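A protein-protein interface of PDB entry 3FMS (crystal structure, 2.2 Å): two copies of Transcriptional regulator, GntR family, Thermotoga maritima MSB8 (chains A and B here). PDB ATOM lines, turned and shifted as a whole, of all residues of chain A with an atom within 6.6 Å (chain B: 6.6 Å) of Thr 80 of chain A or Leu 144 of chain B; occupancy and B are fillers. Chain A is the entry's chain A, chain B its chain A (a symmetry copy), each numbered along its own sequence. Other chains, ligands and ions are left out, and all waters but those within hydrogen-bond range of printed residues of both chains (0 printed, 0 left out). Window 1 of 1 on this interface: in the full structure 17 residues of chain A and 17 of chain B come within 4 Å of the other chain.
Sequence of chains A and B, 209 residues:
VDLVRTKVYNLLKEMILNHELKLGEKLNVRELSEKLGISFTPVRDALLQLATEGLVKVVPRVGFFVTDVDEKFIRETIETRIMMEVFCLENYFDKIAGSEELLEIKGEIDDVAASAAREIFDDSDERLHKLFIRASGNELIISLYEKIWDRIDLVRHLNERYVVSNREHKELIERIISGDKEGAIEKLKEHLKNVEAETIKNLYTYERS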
ATOM      1  N   ARG A  75      20.120 -24.795  26.884  1.00  0.00           N
ATOM      2  CA  ARG A  75      21.098 -24.142  26.014  1.00  0.00           C
ATOM      3  C   ARG A  75      20.501 -23.887  24.646  1.00  0.00           C
ATOM      4  O   ARG A  75      20.585 -22.809  24.147  1.00  0.00           O
ATOM      5  CB  ARG A  75      22.359 -24.990  25.823  1.00  0.00           C
ATOM      6  CG  ARG A  75      23.280 -25.016  27.027  1.00  0.00           C
ATOM      7  CD  ARG A  75      24.680 -25.703  26.728  1.00  0.00           C
ATOM      8  NE  ARG A  75      24.565 -27.103  26.259  1.00  0.00           N
ATOM      9  CZ  ARG A  75      24.779 -28.209  26.991  1.00  0.00           C
ATOM     10  NH1 ARG A  75      25.159 -28.142  28.267  1.00  0.00           N
ATOM     11  NH2 ARG A  75      24.607 -29.398  26.416  1.00  0.00           N
ATOM     12  N   GLU A  76      19.881 -24.900  24.066  1.00  0.00           N
ATOM     13  CA  GLU A  76      19.265 -24.769  22.738  1.00  0.00           C
ATOM     14  C   GLU A  76      18.131 -23.733  22.687  1.00  0.00           C
ATOM     15  O   GLU A  76      18.014 -23.048  21.698  1.00  0.00           O
ATOM     16  CB  GLU A  76      18.786 -26.116  22.223  1.00  0.00           C
ATOM     17  CG  GLU A  76      19.942 -27.106  21.817  1.00  0.00           C
ATOM     18  CD  GLU A  76      19.404 -28.400  21.123  1.00  0.00           C
ATOM     19  OE1 GLU A  76      18.166 -28.595  21.134  1.00  0.00           O
ATOM     20  OE2 GLU A  76      20.190 -29.198  20.561  1.00  0.00           O
ATOM     21  N   THR A  77      17.322 -23.658  23.768  1.00  0.00           N
ATOM     22  CA  THR A  77      16.324 -22.656  23.936  1.00  0.00           C
ATOM     23  C   THR A  77      16.938 -21.277  23.925  1.00  0.00           C
ATOM     24  O   THR A  77      16.503 -20.397  23.181  1.00  0.00           O
ATOM     25  CB  THR A  77      15.506 -22.817  25.219  1.00  0.00           C
ATOM     26  OG1 THR A  77      14.907 -24.105  25.219  1.00  0.00           O
ATOM     27  CG2 THR A  77      14.352 -21.813  25.208  1.00  0.00           C
ATOM     28  N   ILE A  78      17.985 -21.094  24.711  1.00  0.00           N
ATOM     29  CA  ILE A  78      18.572 -19.772  24.822  1.00  0.00           C
ATOM     30  C   ILE A  78      19.303 -19.365  23.536  1.00  0.00           C
ATOM     31  O   ILE A  78      19.235 -18.254  23.096  1.00  0.00           O
ATOM     32  CB  ILE A  78      19.545 -19.741  25.996  1.00  0.00           C
ATOM     33  CG1 ILE A  78      18.799 -20.029  27.290  1.00  0.00           C
ATOM     34  CG2 ILE A  78      20.250 -18.443  26.069  1.00  0.00           C
ATOM     35  CD1 ILE A  78      17.788 -19.044  27.600  1.00  0.00           C
ATOM     36  N   GLU A  79      20.042 -20.287  22.941  1.00  0.00           N
ATOM     37  CA  GLU A  79      20.784 -19.958  21.766  1.00  0.00           C
ATOM     38  C   GLU A  79      19.797 -19.603  20.602  1.00  0.00           C
ATOM     39  O   GLU A  79      20.068 -18.742  19.790  1.00  0.00           O
ATOM     40  CB  GLU A  79      21.697 -21.086  21.358  1.00  0.00           C
ATOM     41  CG  GLU A  79      22.393 -20.820  20.050  1.00  0.00           C
ATOM     42  CD  GLU A  79      23.322 -21.960  19.515  1.00  0.00           C
ATOM     43  OE1 GLU A  79      22.887 -23.128  19.573  1.00  0.00           O
ATOM     44  OE2 GLU A  79      24.456 -21.643  19.015  1.00  0.00           O
ATOM     45  N   THR A  80      18.643 -20.256  20.574  1.00  0.00           N
ATOM     46  CA  THR A  80      17.655 -19.968  19.567  1.00  0.00           C
ATOM     47  C   THR A  80      17.130 -18.526  19.746  1.00  0.00           C
ATOM     48  O   THR A  80      16.962 -17.780  18.759  1.00  0.00           O
ATOM     49  CB  THR A  80      16.514 -20.967  19.560  1.00  0.00           C
ATOM     50  OG1 THR A  80      16.954 -22.254  19.166  1.00  0.00           O
ATOM     51  CG2 THR A  80      15.549 -20.592  18.556  1.00  0.00           C
ATOM     52  N   ARG A  81      16.986 -18.100  21.005  1.00  0.00           N
ATOM     53  CA  ARG A  81      16.487 -16.771  21.314  1.00  0.00           C
ATOM     54  C   ARG A  81      17.532 -15.730  20.940  1.00  0.00           C
ATOM     55  O   ARG A  81      17.202 -14.684  20.392  1.00  0.00           O
ATOM     56  CB  ARG A  81      16.194 -16.672  22.786  1.00  0.00           C
ATOM     57  CG  ARG A  81      14.964 -17.439  23.198  1.00  0.00           C
ATOM     58  CD  ARG A  81      14.698 -17.217  24.677  1.00  0.00           C
ATOM     59  NE  ARG A  81      14.375 -15.839  24.971  1.00  0.00           N
ATOM     60  CZ  ARG A  81      14.160 -15.332  26.181  1.00  0.00           C
ATOM     61  NH1 ARG A  81      14.219 -16.074  27.260  1.00  0.00           N
ATOM     62  NH2 ARG A  81      13.879 -14.046  26.289  1.00  0.00           N
ATOM     63  N   ILE A  82      18.782 -16.049  21.212  1.00  0.00           N
ATOM     64  CA  ILE A  82      19.873 -15.155  20.879  1.00  0.00           C
ATOM     65  C   ILE A  82      19.879 -14.900  19.380  1.00  0.00           C
ATOM     66  O   ILE A  82      19.883 -13.776  18.907  1.00  0.00           O
ATOM     67  CB  ILE A  82      21.244 -15.644  21.347  1.00  0.00           C
ATOM     68  CG1 ILE A  82      21.429 -15.489  22.864  1.00  0.00           C
ATOM     69  CG2 ILE A  82      22.336 -14.825  20.700  1.00  0.00           C
ATOM     70  CD1 ILE A  82      22.620 -16.253  23.360  1.00  0.00           C
ATOM     71  N   MET A  83      19.821 -15.955  18.616  1.00  0.00           N
ATOM     72  CA  MET A  83      19.746 -15.790  17.172  1.00  0.00           C
ATOM     73  C   MET A  83      18.590 -14.868  16.699  1.00  0.00           C
ATOM     74  O   MET A  83      18.734 -13.995  15.843  1.00  0.00           O
ATOM     75  CB  MET A  83      19.540 -17.140  16.606  1.00  0.00           C
ATOM     76  CG  MET A  83      19.043 -17.181  15.211  1.00  0.00           C
ATOM     77  SD  MET A  83      18.717 -18.996  14.460  1.00  0.00           S
ATOM     78  CE  MET A  83      16.985 -19.546  15.054  1.00  0.00           C
ATOM     79  N   MET A  84      17.423 -15.093  17.247  1.00  0.00           N
ATOM     80  CA  MET A  84      16.245 -14.369  16.739  1.00  0.00           C
ATOM     81  C   MET A  84      16.128 -12.966  17.257  1.00  0.00           C
ATOM     82  O   MET A  84      15.865 -12.015  16.486  1.00  0.00           O
ATOM     83  CB  MET A  84      14.980 -15.097  17.085  1.00  0.00           C
ATOM     84  CG  MET A  84      14.925 -16.457  16.454  1.00  0.00           C
ATOM     85  SD  MET A  84      13.272 -17.472  16.777  1.00  0.00           S
ATOM     86  CE  MET A  84      11.970 -16.392  15.830  1.00  0.00           C
ATOM     87  N   GLU A  85      16.317 -12.844  18.557  1.00  0.00           N
ATOM     88  CA  GLU A  85      16.176 -11.554  19.212  1.00  0.00           C
ATOM     89  C   GLU A  85      17.302 -10.597  18.842  1.00  0.00           C
ATOM     90  O   GLU A  85      17.078  -9.418  18.616  1.00  0.00           O
ATOM     91  CB  GLU A  85      16.118 -11.713  20.710  1.00  0.00           C
ATOM     92  CG  GLU A  85      14.863 -12.352  21.204  1.00  0.00           C
ATOM     93  CD  GLU A  85      14.839 -12.464  22.716  1.00  0.00           C
ATOM     94  OE1 GLU A  85      15.385 -11.551  23.357  1.00  0.00           O
ATOM     95  OE2 GLU A  85      14.204 -13.395  23.260  1.00  0.00           O
ATOM     96  N   LEU A 144       7.365 -17.913  14.267  1.00  0.00           N
ATOM     97  CA  LEU A 144       8.292 -18.925  14.769  1.00  0.00           C
ATOM     98  C   LEU A 144       8.487 -18.772  16.294  1.00  0.00           C
ATOM     99  O   LEU A 144       8.451 -19.734  17.053  1.00  0.00           O
ATOM    100  CB  LEU A 144       9.604 -18.871  14.044  1.00  0.00           C
ATOM    101  CG  LEU A 144       9.458 -19.310  12.583  1.00  0.00           C
ATOM    102  CD1 LEU A 144      10.704 -19.055  11.817  1.00  0.00           C
ATOM    103  CD2 LEU A 144       9.114 -20.778  12.462  1.00  0.00           C
ATOM    104  N   TYR A 145       8.570 -17.517  16.728  1.00  0.00           N
ATOM    105  CA  TYR A 145       8.863 -17.222  18.125  1.00  0.00           C
ATOM    106  C   TYR A 145       7.649 -17.598  18.961  1.00  0.00           C
ATOM    107  O   TYR A 145       7.794 -18.162  20.057  1.00  0.00           O
ATOM    108  CB  TYR A 145       9.156 -15.722  18.321  1.00  0.00           C
ATOM    109  CG  TYR A 145       9.838 -15.336  19.596  1.00  0.00           C
ATOM    110  CD1 TYR A 145      11.252 -15.521  19.779  1.00  0.00           C
ATOM    111  CD2 TYR A 145       9.132 -14.681  20.575  1.00  0.00           C
ATOM    112  CE1 TYR A 145      11.873 -15.094  20.946  1.00  0.00           C
ATOM    113  CE2 TYR A 145       9.727 -14.281  21.740  1.00  0.00           C
ATOM    114  CZ  TYR A 145      11.099 -14.502  21.923  1.00  0.00           C
ATOM    115  OH  TYR A 145      11.656 -14.095  23.071  1.00  0.00           O
ATOM    116  N   LYS A 147       5.423 -19.795  18.171  1.00  0.00           N
ATOM    117  CA  LYS A 147       5.380 -21.245  18.197  1.00  0.00           C
ATOM    118  C   LYS A 147       6.206 -21.898  19.348  1.00  0.00           C
ATOM    119  O   LYS A 147       5.897 -22.964  19.809  1.00  0.00           O
ATOM    120  CB  LYS A 147       5.910 -21.751  16.864  1.00  0.00           C
ATOM    121  CG  LYS A 147       5.635 -23.236  16.534  1.00  0.00           C
ATOM    122  CD  LYS A 147       5.781 -23.551  14.968  1.00  0.00           C
ATOM    123  CE  LYS A 147       4.846 -22.689  13.998  1.00  0.00           C
ATOM    124  NZ  LYS A 147       4.861 -23.082  12.521  1.00  0.00           N
ATOM    125  N   ILE A 148       7.251 -21.241  19.810  1.00  0.00           N
ATOM    126  CA  ILE A 148       8.095 -21.822  20.810  1.00  0.00           C
ATOM    127  C   ILE A 148       8.006 -21.036  22.084  1.00  0.00           C
ATOM    128  O   ILE A 148       8.782 -21.246  23.009  1.00  0.00           O
ATOM    129  CB  ILE A 148       9.549 -21.857  20.374  1.00  0.00           C
ATOM    130  CG1 ILE A 148      10.070 -20.492  20.007  1.00  0.00           C
ATOM    131  CG2 ILE A 148       9.722 -22.759  19.186  1.00  0.00           C
ATOM    132  CD1 ILE A 148      11.579 -20.469  19.805  1.00  0.00           C
ATOM    133  N   MET B  84      18.767 -17.092  10.141  1.00  0.00           N
ATOM    134  CA  MET B  84      19.143 -18.416  10.666  1.00  0.00           C
ATOM    135  C   MET B  84      20.440 -18.936  10.123  1.00  0.00           C
ATOM    136  O   MET B  84      21.299 -19.442  10.881  1.00  0.00           O
ATOM    137  CB  MET B  84      18.077 -19.430  10.369  1.00  0.00           C
ATOM    138  CG  MET B  84      16.775 -19.084  11.028  1.00  0.00           C
ATOM    139  SD  MET B  84      15.326 -20.389  10.771  1.00  0.00           S
ATOM    140  CE  MET B  84      16.019 -21.923  11.730  1.00  0.00           C
ATOM    141  N   PHE B  87      23.413 -16.772  11.212  1.00  0.00           N
ATOM    142  CA  PHE B  87      23.714 -17.085  12.596  1.00  0.00           C
ATOM    143  C   PHE B  87      24.498 -18.402  12.675  1.00  0.00           C
ATOM    144  O   PHE B  87      25.478 -18.470  13.396  1.00  0.00           O
ATOM    145  CB  PHE B  87      22.461 -17.162  13.444  1.00  0.00           C
ATOM    146  CG  PHE B  87      22.709 -17.522  14.870  1.00  0.00           C
ATOM    147  CD1 PHE B  87      22.952 -16.535  15.817  1.00  0.00           C
ATOM    148  CD2 PHE B  87      22.737 -18.839  15.273  1.00  0.00           C
ATOM    149  CE1 PHE B  87      23.183 -16.868  17.174  1.00  0.00           C
ATOM    150  CE2 PHE B  87      22.994 -19.178  16.625  1.00  0.00           C
ATOM    151  CZ  PHE B  87      23.208 -18.151  17.571  1.00  0.00           C
ATOM    152  N   ASN B 138      22.062 -27.773  16.956  1.00  0.00           N
ATOM    153  CA  ASN B 138      21.001 -27.273  17.823  1.00  0.00           C
ATOM    154  C   ASN B 138      19.695 -27.808  17.200  1.00  0.00           C
ATOM    155  O   ASN B 138      19.244 -27.384  16.178  1.00  0.00           O
ATOM    156  CB  ASN B 138      21.047 -25.757  17.860  1.00  0.00           C
ATOM    157  CG  ASN B 138      19.976 -25.179  18.680  1.00  0.00           C
ATOM    158  OD1 ASN B 138      18.846 -25.697  18.736  1.00  0.00           O
ATOM    159  ND2 ASN B 138      20.337 -24.135  19.402  1.00  0.00           N
ATOM    160  N   GLU B 139      19.124 -28.792  17.847  1.00  0.00           N
ATOM    161  CA  GLU B 139      18.029 -29.483  17.295  1.00  0.00           C
ATOM    162  C   GLU B 139      16.757 -28.623  17.216  1.00  0.00           C
ATOM    163  O   GLU B 139      15.930 -28.896  16.408  1.00  0.00           O
ATOM    164  CB  GLU B 139      17.791 -30.713  18.143  1.00  0.00           C
ATOM    165  CG  GLU B 139      18.719 -31.903  17.741  1.00  0.00           C
ATOM    166  CD  GLU B 139      18.723 -33.062  18.773  1.00  0.00           C
ATOM    167  OE1 GLU B 139      17.740 -33.224  19.566  1.00  0.00           O
ATOM    168  OE2 GLU B 139      19.742 -33.800  18.793  1.00  0.00           O
ATOM    169  N   LEU B 140      16.660 -27.584  18.029  1.00  0.00           N
ATOM    170  CA  LEU B 140      15.498 -26.644  17.972  1.00  0.00           C
ATOM    171  C   LEU B 140      15.651 -25.856  16.700  1.00  0.00           C
ATOM    172  O   LEU B 140      14.714 -25.761  15.940  1.00  0.00           O
ATOM    173  CB  LEU B 140      15.500 -25.678  19.146  1.00  0.00           C
ATOM    174  CG  LEU B 140      14.234 -25.214  19.862  1.00  0.00           C
ATOM    175  CD1 LEU B 140      14.461 -23.932  20.606  1.00  0.00           C
ATOM    176  CD2 LEU B 140      13.157 -25.124  18.908  1.00  0.00           C
ATOM    177  N   ILE B 141      16.845 -25.288  16.496  1.00  0.00           N
ATOM    178  CA  ILE B 141      17.120 -24.538  15.265  1.00  0.00           C
ATOM    179  C   ILE B 141      16.865 -25.337  14.040  1.00  0.00           C
ATOM    180  O   ILE B 141      16.177 -24.874  13.083  1.00  0.00           O
ATOM    181  CB  ILE B 141      18.547 -23.949  15.222  1.00  0.00           C
ATOM    182  CG1 ILE B 141      18.656 -22.784  16.205  1.00  0.00           C
ATOM    183  CG2 ILE B 141      18.818 -23.362  13.872  1.00  0.00           C
ATOM    184  CD1 ILE B 141      20.094 -22.276  16.434  1.00  0.00           C
ATOM    185  N   ILE B 142      17.436 -26.532  14.051  1.00  0.00           N
ATOM    186  CA  ILE B 142      17.362 -27.429  12.877  1.00  0.00           C
ATOM    187  C   ILE B 142      15.897 -27.799  12.603  1.00  0.00           C
ATOM    188  O   ILE B 142      15.489 -27.828  11.477  1.00  0.00           O
ATOM    189  CB  ILE B 142      18.185 -28.734  13.099  1.00  0.00           C
ATOM    190  CG1 ILE B 142      19.704 -28.484  12.997  1.00  0.00           C
ATOM    191  CG2 ILE B 142      17.674 -29.889  12.183  1.00  0.00           C
ATOM    192  CD1 ILE B 142      20.620 -29.646  13.741  1.00  0.00           C
ATOM    193  N   SER B 143      15.097 -28.010  13.645  1.00  0.00           N
ATOM    194  CA  SER B 143      13.664 -28.310  13.472  1.00  0.00           C
ATOM    195  C   SER B 143      12.860 -27.056  13.054  1.00  0.00           C
ATOM    196  O   SER B 143      11.918 -27.139  12.301  1.00  0.00           O
ATOM    197  CB  SER B 143      13.068 -28.831  14.775  1.00  0.00           C
ATOM    198  OG  SER B 143      13.156 -27.884  15.823  1.00  0.00           O
ATOM    199  N   LEU B 144      13.300 -25.877  13.446  1.00  0.00           N
ATOM    200  CA  LEU B 144      12.579 -24.711  12.941  1.00  0.00           C
ATOM    201  C   LEU B 144      12.740 -24.598  11.408  1.00  0.00           C
ATOM    202  O   LEU B 144      11.787 -24.375  10.670  1.00  0.00           O
ATOM    203  CB  LEU B 144      13.021 -23.454  13.629  1.00  0.00           C
ATOM    204  CG  LEU B 144      12.599 -23.440  15.102  1.00  0.00           C
ATOM    205  CD1 LEU B 144      13.216 -22.303  15.828  1.00  0.00           C
ATOM    206  CD2 LEU B 144      11.096 -23.352  15.261  1.00  0.00           C
ATOM    207  N   TYR B 145      13.955 -24.883  10.947  1.00  0.00           N
ATOM    208  CA  TYR B 145      14.283 -24.713   9.537  1.00  0.00           C
ATOM    209  C   TYR B 145      13.557 -25.788   8.742  1.00  0.00           C
ATOM    210  O   TYR B 145      13.028 -25.511   7.653  1.00  0.00           O
ATOM    211  CB  TYR B 145      15.798 -24.862   9.303  1.00  0.00           C
ATOM    212  CG  TYR B 145      16.327 -24.342   8.002  1.00  0.00           C
ATOM    213  CD1 TYR B 145      16.545 -22.938   7.785  1.00  0.00           C
ATOM    214  CD2 TYR B 145      16.730 -25.224   7.029  1.00  0.00           C
ATOM    215  CE1 TYR B 145      17.098 -22.487   6.594  1.00  0.00           C
ATOM    216  CE2 TYR B 145      17.250 -24.791   5.841  1.00  0.00           C
ATOM    217  CZ  TYR B 145      17.420 -23.416   5.626  1.00  0.00           C
ATOM    218  OH  TYR B 145      17.938 -23.020   4.455  1.00  0.00           O
ATOM    219  N   GLU B 146      13.615 -27.028   9.262  1.00  0.00           N
ATOM    220  CA  GLU B 146      12.884 -28.150   8.683  1.00  0.00           C
ATOM    221  C   GLU B 146      11.396 -27.886   8.588  1.00  0.00           C
ATOM    222  O   GLU B 146      10.793 -28.147   7.547  1.00  0.00           O
ATOM    223  CB  GLU B 146      13.155 -29.491   9.413  1.00  0.00           C
ATOM    224  CG  GLU B 146      13.127 -30.756   8.447  1.00  0.00           C
ATOM    225  CD  GLU B 146      14.080 -30.656   7.203  1.00  0.00           C
ATOM    226  OE1 GLU B 146      15.310 -30.417   7.382  1.00  0.00           O
ATOM    227  OE2 GLU B 146      13.591 -30.824   6.041  1.00  0.00           O
ATOM    228  N   LYS B 147      10.842 -27.284   9.635  1.00  0.00           N
ATOM    229  CA  LYS B 147       9.439 -26.916   9.640  1.00  0.00           C
ATOM    230  C   LYS B 147       9.016 -25.961   8.480  1.00  0.00           C
ATOM    231  O   LYS B 147       7.893 -25.965   8.049  1.00  0.00           O
ATOM    232  CB  LYS B 147       9.140 -26.237  10.968  1.00  0.00           C
ATOM    233  CG  LYS B 147       7.646 -26.073  11.335  1.00  0.00           C
ATOM    234  CD  LYS B 147       7.428 -25.813  12.902  1.00  0.00           C
ATOM    235  CE  LYS B 147       8.017 -26.933  13.879  1.00  0.00           C
ATOM    236  NZ  LYS B 147       7.683 -26.778  15.363  1.00  0.00           N
ATOM    237  N   ILE B 148       9.929 -25.155   7.977  1.00  0.00           N
ATOM    238  CA  ILE B 148       9.583 -24.201   6.967  1.00  0.00           C
ATOM    239  C   ILE B 148      10.277 -24.535   5.680  1.00  0.00           C
ATOM    240  O   ILE B 148      10.270 -23.750   4.738  1.00  0.00           O
ATOM    241  CB  ILE B 148       9.972 -22.788   7.364  1.00  0.00           C
ATOM    242  CG1 ILE B 148      11.438 -22.668   7.689  1.00  0.00           C
ATOM    243  CG2 ILE B 148       9.189 -22.343   8.564  1.00  0.00           C
ATOM    244  CD1 ILE B 148      11.892 -21.223   7.850  1.00  0.00           C
ATOM    245  N   TRP B 149      10.802 -25.748   5.614  1.00  0.00           N
ATOM    246  CA  TRP B 149      11.619 -26.132   4.465  1.00  0.00           C
ATOM    247  C   TRP B 149      10.756 -26.116   3.207  1.00  0.00           C
ATOM    248  O   TRP B 149      11.198 -25.651   2.207  1.00  0.00           O
ATOM    249  CB  TRP B 149      12.253 -27.526   4.600  1.00  0.00           C
ATOM    250  CG  TRP B 149      12.969 -27.867   3.367  1.00  0.00           C
ATOM    251  CD1 TRP B 149      12.589 -28.799   2.493  1.00  0.00           C
ATOM    252  CD2 TRP B 149      14.074 -27.161   2.750  1.00  0.00           C
ATOM    253  NE1 TRP B 149      13.394 -28.778   1.372  1.00  0.00           N
ATOM    254  CE2 TRP B 149      14.302 -27.751   1.499  1.00  0.00           C
ATOM    255  CE3 TRP B 149      14.858 -26.063   3.112  1.00  0.00           C
ATOM    256  CZ2 TRP B 149      15.331 -27.324   0.611  1.00  0.00           C
ATOM    257  CZ3 TRP B 149      15.913 -25.625   2.199  1.00  0.00           C
ATOM    258  CH2 TRP B 149      16.119 -26.257   0.991  1.00  0.00           C
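The backbone carbonyl oxygen (O) of Glu 76 of chain A sits at hydrogen-bond distance from the side-chain amide nitrogen (ND2) of Asn 138 of chain B (3.4 Å). The backbone NH of Glu 139 of chain B lies within hydrogen-bond range of the side-chain carboxylate of Glu 76 of chain A (2.9 Å). The side-chain carboxylate (OE1) of Glu 79 of chain A sits at hydrogen-bond distance from the side-chain amide nitrogen (ND2) of Asn 138 of chain B.
OD1 of Asn 138 of chain B lies within hydrogen-bond range of N of Ile 141 of chain B (3.0 Å). The backbone carbonyl oxygen (O) of Glu 76 of chain A is in hydrogen-bond range of the side-chain hydroxyl (OG1) of Thr 80 of chain A, 2.9 Å away. OG of Ser 143 of chain B sits at hydrogen-bond distance from O of Leu 140 of chain B (2.6 Å). OG of Ser 143 of chain B sits at hydrogen-bond distance from O of Glu 139 of chain B, 3.0 Å away. The backbone NH (N) of Leu 140 of chain B lies within hydrogen-bond range of the side-chain amide oxygen (OD1) of Asn 138 of chain B (3.0 Å).
Leu 140 of chain B touches Glu 76 of chain A. Glu 79 of chain A touches Phe 87 of chain B (OE2 to CE2, 3.7 Å). Asn 138 of chain B touches Thr 80 of chain A (ND2 to OG1, 3.9 Å). Leu 140 of chain B touches Thr 80 of chain A (CD1 to OG1, 3.3 Å). Thr 80 of chain A touches Ile 141 of chain B (OG1 to CG1, 3.5 Å). Thr 80 of chain A touches Leu 144 of chain B. Met 83 of chain A touches Met 84 of chain B (SD to CA, 3.9 Å). Phe 87 of chain B touches Met 83 of chain A (CD1 to CB, 3.6 Å). Met 83 of chain A touches Ile 141 of chain B. CD of Lys 147 of chain A touches CD of Lys 147 of chain B (3.5 Å).
Leu 144 of chain B touches just one residue of chain A: Thr 80 (3.98 Å). Of the printed residues of chain B, Glu 79 of chain A touches Phe 87 and Asn 138. Of the printed residues of chain A, Phe 87 of chain B touches Glu 79 (3.7 Å) and Met 83 (3.6 Å). Printed residues of chain A within 4 Å of Glu 139 of chain B: Glu 76. Printed residues of chain B within 4 Å of Met 83 of chain A: Met 84 (3.9 Å), Phe 87 (3.6 Å) and Ile 141 (3.8 Å). Printed residues of chain A within 4 Å of Met 84 of chain B: Met 83. The nearest residue of chain A that does not touch Leu 144 of chain B is Ile 148 of chain A (4.2 Å).
Of the 14 printed residues of chain B, 8 touch a printed residue of chain A. Hydrophobic or aromatic side chains of chain A within 4 Å of the printed part of chain B: Met 83.
Lys 147 of chain B touches its own counterpart, Lys 147 of chain A. 5 positions are printed for both chains. Of the 13 pairs that touch across the chains among the printed residues, 1 has its exchanged pair printed and touching as well.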
